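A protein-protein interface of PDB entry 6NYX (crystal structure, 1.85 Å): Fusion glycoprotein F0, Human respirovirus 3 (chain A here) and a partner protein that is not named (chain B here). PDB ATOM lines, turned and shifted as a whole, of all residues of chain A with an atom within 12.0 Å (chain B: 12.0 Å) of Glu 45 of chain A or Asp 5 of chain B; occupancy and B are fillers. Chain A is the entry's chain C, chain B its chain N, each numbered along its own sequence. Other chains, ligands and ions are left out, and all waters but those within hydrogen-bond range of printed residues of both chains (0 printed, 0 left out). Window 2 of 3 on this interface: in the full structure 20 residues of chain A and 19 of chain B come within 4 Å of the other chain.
Among the printed residues, merely in contact across the chains: Ser 37 of chain A with Ile 9 of chain B (3.1 Å), Val 38 of chain A with Ile 7 of chain B (3.9 Å), Val 38 of chain A with Ile 9 of chain B (3.9 Å), Tyr 41 of chain A with Pro 6 of chain B (3.7 Å), Tyr 41 of chain A with Ile 7 of chain B (3.5 Å) and Glu 45 of chain A with Asp 5 of chain B (3.96 Å).
The side-chain hydroxyl of Tyr 41 of chain A sits at hydrogen-bond distance from the backbone carbonyl oxygen of Asp 5 of chain B (2.6 Å).
Of the printed residues of chain B, Ser 37 of chain A touches Ile 9.
Printed residues of chain B within 4 Å of Val 38 of chain A: Ile 7 (3.9 Å) and Ile 9 (3.9 Å).
Tyr 41 of chain A touches just these residues of chain B: Asp 5 (2.6 Å), Pro 6 (3.7 Å) and Ile 7 (3.5 Å).
No residue of chain B comes within 4 Å of Val 42 of chain A.
Asn 43 of chain A touches none of the printed residues of chain B.
No residue of chain B comes within 4 Å of Lys 44 of chain A.
Of chain B, only Asp 5 comes within 4 Å of Glu 45 of chain A.
No residue of chain B comes within 4 Å of Pro 48 of chain A.
No residue of chain A comes within 4 Å of Leu 4 of chain B.
Ile 7 of chain B touches just these residues of chain A: Val 38 and Tyr 41.
Printed residues of chain A within 4 Å of Ile 9 of chain B: Ser 37 (3.1 Å) and Val 38 (3.9 Å).
The nearest printed residue of chain B that does not touch Ser 37 of chain A is Ile 7 of chain B (4.4 Å).
Printed residues of chain A that touch a printed residue of chain B: Ser 37, Val 38, Tyr 41 and Glu 45.
Hydrophobic or aromatic side chains of chain A within 4 Å of the printed part of chain B: Val 38 and Tyr 41.
Of the 6 printed residues of chain B, 4 touch a printed residue of chain A.
Printed residues of chain B that touch a printed residue of chain A: Asp 5, Pro 6, Ile 7 and Ile 9.
Among the printed residues, 7 pairs touch across the chains.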
ATOM      1  N   LYS A  36      28.293  -6.003  -3.858  1.00  0.00           N
ATOM      2  CA  LYS A  36      28.913  -7.258  -3.381  1.00  0.00           C
ATOM      3  C   LYS A  36      28.291  -7.650  -2.037  1.00  0.00           C
ATOM      4  O   LYS A  36      28.035  -8.826  -1.840  1.00  0.00           O
ATOM      5  CB  LYS A  36      30.427  -7.118  -3.287  1.00  0.00           C
ATOM      6  CG  LYS A  36      31.142  -8.397  -2.909  1.00  0.00           C
ATOM      7  CD  LYS A  36      32.575  -8.169  -2.457  1.00  0.00           C
ATOM      8  CE  LYS A  36      33.214  -9.377  -1.803  1.00  0.00           C
ATOM      9  NZ  LYS A  36      32.510 -10.637  -2.142  1.00  0.00           N
ATOM     10  N   SER A  37      28.067  -6.684  -1.150  1.00  0.00           N
ATOM     11  CA  SER A  37      27.462  -6.883   0.183  1.00  0.00           C
ATOM     12  C   SER A  37      26.025  -7.367   0.021  1.00  0.00           C
ATOM     13  O   SER A  37      25.607  -8.167   0.829  1.00  0.00           O
ATOM     14  CB  SER A  37      27.558  -5.670   1.024  1.00  0.00           C
ATOM     15  OG  SER A  37      26.476  -4.824   0.772  1.00  0.00           O
ATOM     16  N   VAL A  38      25.325  -6.970  -1.032  1.00  0.00           N
ATOM     17  CA  VAL A  38      23.937  -7.447  -1.289  1.00  0.00           C
ATOM     18  C   VAL A  38      24.019  -8.905  -1.745  1.00  0.00           C
ATOM     19  O   VAL A  38      23.228  -9.690  -1.274  1.00  0.00           O
ATOM     20  CB  VAL A  38      23.204  -6.562  -2.309  1.00  0.00           C
ATOM     21  CG1 VAL A  38      21.969  -7.240  -2.867  1.00  0.00           C
ATOM     22  CG2 VAL A  38      22.860  -5.212  -1.714  1.00  0.00           C
ATOM     23  N   GLN A  39      24.969  -9.244  -2.616  1.00  0.00           N
ATOM     24  CA  GLN A  39      25.179 -10.626  -3.117  1.00  0.00           C
ATOM     25  C   GLN A  39      25.532 -11.495  -1.915  1.00  0.00           C
ATOM     26  O   GLN A  39      24.960 -12.556  -1.770  1.00  0.00           O
ATOM     27  CB  GLN A  39      26.277 -10.685  -4.179  1.00  0.00           C
ATOM     28  CG  GLN A  39      26.787 -12.080  -4.500  1.00  0.00           C
ATOM     29  CD  GLN A  39      28.222 -12.041  -4.964  1.00  0.00           C
ATOM     30  OE1 GLN A  39      28.526 -12.186  -6.128  1.00  0.00           O
ATOM     31  NE2 GLN A  39      29.123 -11.781  -4.041  1.00  0.00           N
ATOM     32  N   ASP A  40      26.432 -11.029  -1.071  1.00  0.00           N
ATOM     33  CA  ASP A  40      26.862 -11.790   0.121  1.00  0.00           C
ATOM     34  C   ASP A  40      25.622 -12.029   0.997  1.00  0.00           C
ATOM     35  O   ASP A  40      25.339 -13.174   1.298  1.00  0.00           O
ATOM     36  CB  ASP A  40      28.038 -11.105   0.816  1.00  0.00           C
ATOM     37  CG  ASP A  40      29.351 -11.149   0.048  1.00  0.00           C
ATOM     38  OD1 ASP A  40      29.414 -11.822  -0.964  1.00  0.00           O
ATOM     39  OD2 ASP A  40      30.285 -10.494   0.478  1.00  0.00           O
ATOM     40  N   TYR A  41      24.853 -11.003   1.337  1.00  0.00           N
ATOM     41  CA  TYR A  41      23.702 -11.175   2.219  1.00  0.00           C
ATOM     42  C   TYR A  41      22.722 -12.182   1.642  1.00  0.00           C
ATOM     43  O   TYR A  41      22.184 -13.027   2.362  1.00  0.00           O
ATOM     44  CB  TYR A  41      23.008  -9.828   2.434  1.00  0.00           C
ATOM     45  CG  TYR A  41      21.736  -9.874   3.248  1.00  0.00           C
ATOM     46  CD1 TYR A  41      21.755  -9.638   4.603  1.00  0.00           C
ATOM     47  CD2 TYR A  41      20.512 -10.120   2.644  1.00  0.00           C
ATOM     48  CE1 TYR A  41      20.587  -9.674   5.357  1.00  0.00           C
ATOM     49  CE2 TYR A  41      19.346 -10.167   3.387  1.00  0.00           C
ATOM     50  CZ  TYR A  41      19.393  -9.922   4.744  1.00  0.00           C
ATOM     51  OH  TYR A  41      18.235  -9.960   5.491  1.00  0.00           O
ATOM     52  N   VAL A  42      22.460 -12.094   0.347  1.00  0.00           N
ATOM     53  CA  VAL A  42      21.581 -13.057  -0.307  1.00  0.00           C
ATOM     54  C   VAL A  42      22.110 -14.477  -0.134  1.00  0.00           C
ATOM     55  O   VAL A  42      21.366 -15.396   0.228  1.00  0.00           O
ATOM     56  CB  VAL A  42      21.429 -12.692  -1.790  1.00  0.00           C
ATOM     57  CG1 VAL A  42      20.716 -13.778  -2.551  1.00  0.00           C
ATOM     58  CG2 VAL A  42      20.685 -11.372  -1.935  1.00  0.00           C
ATOM     59  N   ASN A  43      23.400 -14.682  -0.392  1.00  0.00           N
ATOM     60  CA  ASN A  43      23.954 -16.034  -0.382  1.00  0.00           C
ATOM     61  C   ASN A  43      24.202 -16.555   1.034  1.00  0.00           C
ATOM     62  O   ASN A  43      24.170 -17.772   1.251  1.00  0.00           O
ATOM     63  CB  ASN A  43      25.246 -16.071  -1.215  1.00  0.00           C
ATOM     64  CG  ASN A  43      24.977 -16.028  -2.740  1.00  0.00           C
ATOM     65  OD1 ASN A  43      23.894 -16.365  -3.195  1.00  0.00           O
ATOM     66  ND2 ASN A  43      25.979 -15.627  -3.521  1.00  0.00           N
ATOM     67  N   LYS A  44      24.408 -15.666   2.007  1.00  0.00           N
ATOM     68  CA  LYS A  44      24.732 -16.099   3.357  1.00  0.00           C
ATOM     69  C   LYS A  44      23.513 -16.225   4.256  1.00  0.00           C
ATOM     70  O   LYS A  44      23.574 -16.953   5.254  1.00  0.00           O
ATOM     71  CB  LYS A  44      25.712 -15.123   4.020  1.00  0.00           C
ATOM     72  N   GLU A  45      22.374 -15.637   3.852  1.00  0.00           N
ATOM     73  CA  GLU A  45      21.158 -15.571   4.703  1.00  0.00           C
ATOM     74  C   GLU A  45      19.843 -15.911   4.005  1.00  0.00           C
ATOM     75  O   GLU A  45      19.112 -16.655   4.585  1.00  0.00           O
ATOM     76  CB  GLU A  45      21.049 -14.189   5.313  1.00  0.00           C
ATOM     77  CG  GLU A  45      22.375 -13.681   5.796  1.00  0.00           C
ATOM     78  CD  GLU A  45      22.349 -13.141   7.200  1.00  0.00           C
ATOM     79  OE1 GLU A  45      21.289 -12.684   7.633  1.00  0.00           O
ATOM     80  OE2 GLU A  45      23.377 -13.206   7.860  1.00  0.00           O
ATOM     81  N   ILE A  46      19.494 -15.379   2.845  1.00  0.00           N
ATOM     82  CA  ILE A  46      18.172 -15.699   2.243  1.00  0.00           C
ATOM     83  C   ILE A  46      18.210 -17.076   1.589  1.00  0.00           C
ATOM     84  O   ILE A  46      17.289 -17.829   1.809  1.00  0.00           O
ATOM     85  CB  ILE A  46      17.737 -14.610   1.265  1.00  0.00           C
ATOM     86  CG1 ILE A  46      17.892 -13.238   1.906  1.00  0.00           C
ATOM     87  CG2 ILE A  46      16.336 -14.832   0.732  1.00  0.00           C
ATOM     88  CD1 ILE A  46      17.667 -12.129   0.947  1.00  0.00           C
ATOM     89  N   VAL A  47      19.217 -17.389   0.793  1.00  0.00           N
ATOM     90  CA  VAL A  47      19.285 -18.677   0.058  1.00  0.00           C
ATOM     91  C   VAL A  47      19.068 -19.842   1.022  1.00  0.00           C
ATOM     92  O   VAL A  47      18.183 -20.645   0.750  1.00  0.00           O
ATOM     93  CB  VAL A  47      20.611 -18.828  -0.691  1.00  0.00           C
ATOM     94  CG1 VAL A  47      20.818 -20.269  -1.115  1.00  0.00           C
ATOM     95  CG2 VAL A  47      20.659 -17.895  -1.881  1.00  0.00           C
ATOM     96  N   PRO A  48      19.873 -20.037   2.082  1.00  0.00           N
ATOM     97  CA  PRO A  48      19.628 -21.160   2.995  1.00  0.00           C
ATOM     98  C   PRO A  48      18.245 -21.205   3.666  1.00  0.00           C
ATOM     99  O   PRO A  48      17.693 -22.251   3.797  1.00  0.00           O
ATOM    100  CB  PRO A  48      20.676 -20.984   4.098  1.00  0.00           C
ATOM    101  CG  PRO A  48      21.133 -19.575   3.936  1.00  0.00           C
ATOM    102  CD  PRO A  48      21.119 -19.380   2.447  1.00  0.00           C
ATOM    103  N   SER A  49      17.687 -20.071   4.059  1.00  0.00           N
ATOM    104  CA  SER A  49      16.355 -20.005   4.705  1.00  0.00           C
ATOM    105  C   SER A  49      15.319 -20.648   3.793  1.00  0.00           C
ATOM    106  O   SER A  49      14.502 -21.387   4.305  1.00  0.00           O
ATOM    107  CB  SER A  49      15.959 -18.601   5.032  1.00  0.00           C
ATOM    108  N   ILE A  50      15.342 -20.323   2.501  1.00  0.00           N
ATOM    109  CA  ILE A  50      14.415 -20.847   1.462  1.00  0.00           C
ATOM    110  C   ILE A  50      14.953 -22.193   0.987  1.00  0.00           C
ATOM    111  O   ILE A  50      14.627 -22.559  -0.144  1.00  0.00           O
ATOM    112  CB  ILE A  50      14.271 -19.851   0.296  1.00  0.00           C
ATOM    113  N   LEU B   4      15.058 -13.711   9.149  1.00  0.00           N
ATOM    114  CA  LEU B   4      16.490 -13.372   8.941  1.00  0.00           C
ATOM    115  C   LEU B   4      16.725 -11.944   9.409  1.00  0.00           C
ATOM    116  O   LEU B   4      15.779 -11.195   9.365  1.00  0.00           O
ATOM    117  CB  LEU B   4      16.808 -13.519   7.456  1.00  0.00           C
ATOM    118  N   ASP B   5      17.915 -11.595   9.891  1.00  0.00           N
ATOM    119  CA  ASP B   5      18.197 -10.203  10.331  1.00  0.00           C
ATOM    120  C   ASP B   5      18.220  -9.303   9.080  1.00  0.00           C
ATOM    121  O   ASP B   5      18.654  -9.761   8.039  1.00  0.00           O
ATOM    122  CB  ASP B   5      19.447 -10.155  11.203  1.00  0.00           C
ATOM    123  N   PRO B   6      17.733  -8.049   9.123  1.00  0.00           N
ATOM    124  CA  PRO B   6      17.683  -7.208   7.933  1.00  0.00           C
ATOM    125  C   PRO B   6      19.017  -6.648   7.432  1.00  0.00           C
ATOM    126  O   PRO B   6      19.848  -6.281   8.217  1.00  0.00           O
ATOM    127  CB  PRO B   6      16.789  -6.042   8.339  1.00  0.00           C
ATOM    128  CG  PRO B   6      16.892  -5.989   9.834  1.00  0.00           C
ATOM    129  CD  PRO B   6      17.140  -7.406  10.277  1.00  0.00           C
ATOM    130  N   ILE B   7      19.157  -6.621   6.115  1.00  0.00           N
ATOM    131  CA  ILE B   7      20.338  -6.072   5.409  1.00  0.00           C
ATOM    132  C   ILE B   7      20.369  -4.565   5.667  1.00  0.00           C
ATOM    133  O   ILE B   7      19.330  -3.947   5.647  1.00  0.00           O
ATOM    134  CB  ILE B   7      20.269  -6.402   3.909  1.00  0.00           C
ATOM    135  CG1 ILE B   7      21.573  -6.065   3.193  1.00  0.00           C
ATOM    136  CG2 ILE B   7      19.094  -5.703   3.273  1.00  0.00           C
ATOM    137  CD1 ILE B   7      21.634  -6.542   1.782  1.00  0.00           C
ATOM    138  N   ASP B   8      21.530  -3.984   5.902  1.00  0.00           N
ATOM    139  CA  ASP B   8      21.633  -2.531   6.151  1.00  0.00           C
ATOM    140  C   ASP B   8      22.917  -2.019   5.512  1.00  0.00           C
ATOM    141  O   ASP B   8      23.935  -2.144   6.138  1.00  0.00           O
ATOM    142  CB  ASP B   8      21.664  -2.196   7.630  1.00  0.00           C
ATOM    143  CG  ASP B   8      21.734  -0.711   7.896  1.00  0.00           C
ATOM    144  OD1 ASP B   8      21.835   0.046   6.962  1.00  0.00           O
ATOM    145  OD2 ASP B   8      21.710  -0.352   9.031  1.00  0.00           O
ATOM    146  N   ILE B   9      22.842  -1.511   4.291  1.00  0.00           N
ATOM    147  CA  ILE B   9      24.018  -0.972   3.564  1.00  0.00           C
ATOM    148  C   ILE B   9      23.975   0.550   3.609  1.00  0.00           C
ATOM    149  O   ILE B   9      24.591   1.157   2.801  1.00  0.00           O
ATOM    150  CB  ILE B   9      24.035  -1.509   2.129  1.00  0.00           C
ATOM    151  CG1 ILE B   9      22.707  -1.246   1.453  1.00  0.00           C
ATOM    152  CG2 ILE B   9      24.392  -2.973   2.087  1.00  0.00           C
ATOM    153  CD1 ILE B   9      22.663  -1.739   0.060  1.00  0.00           C
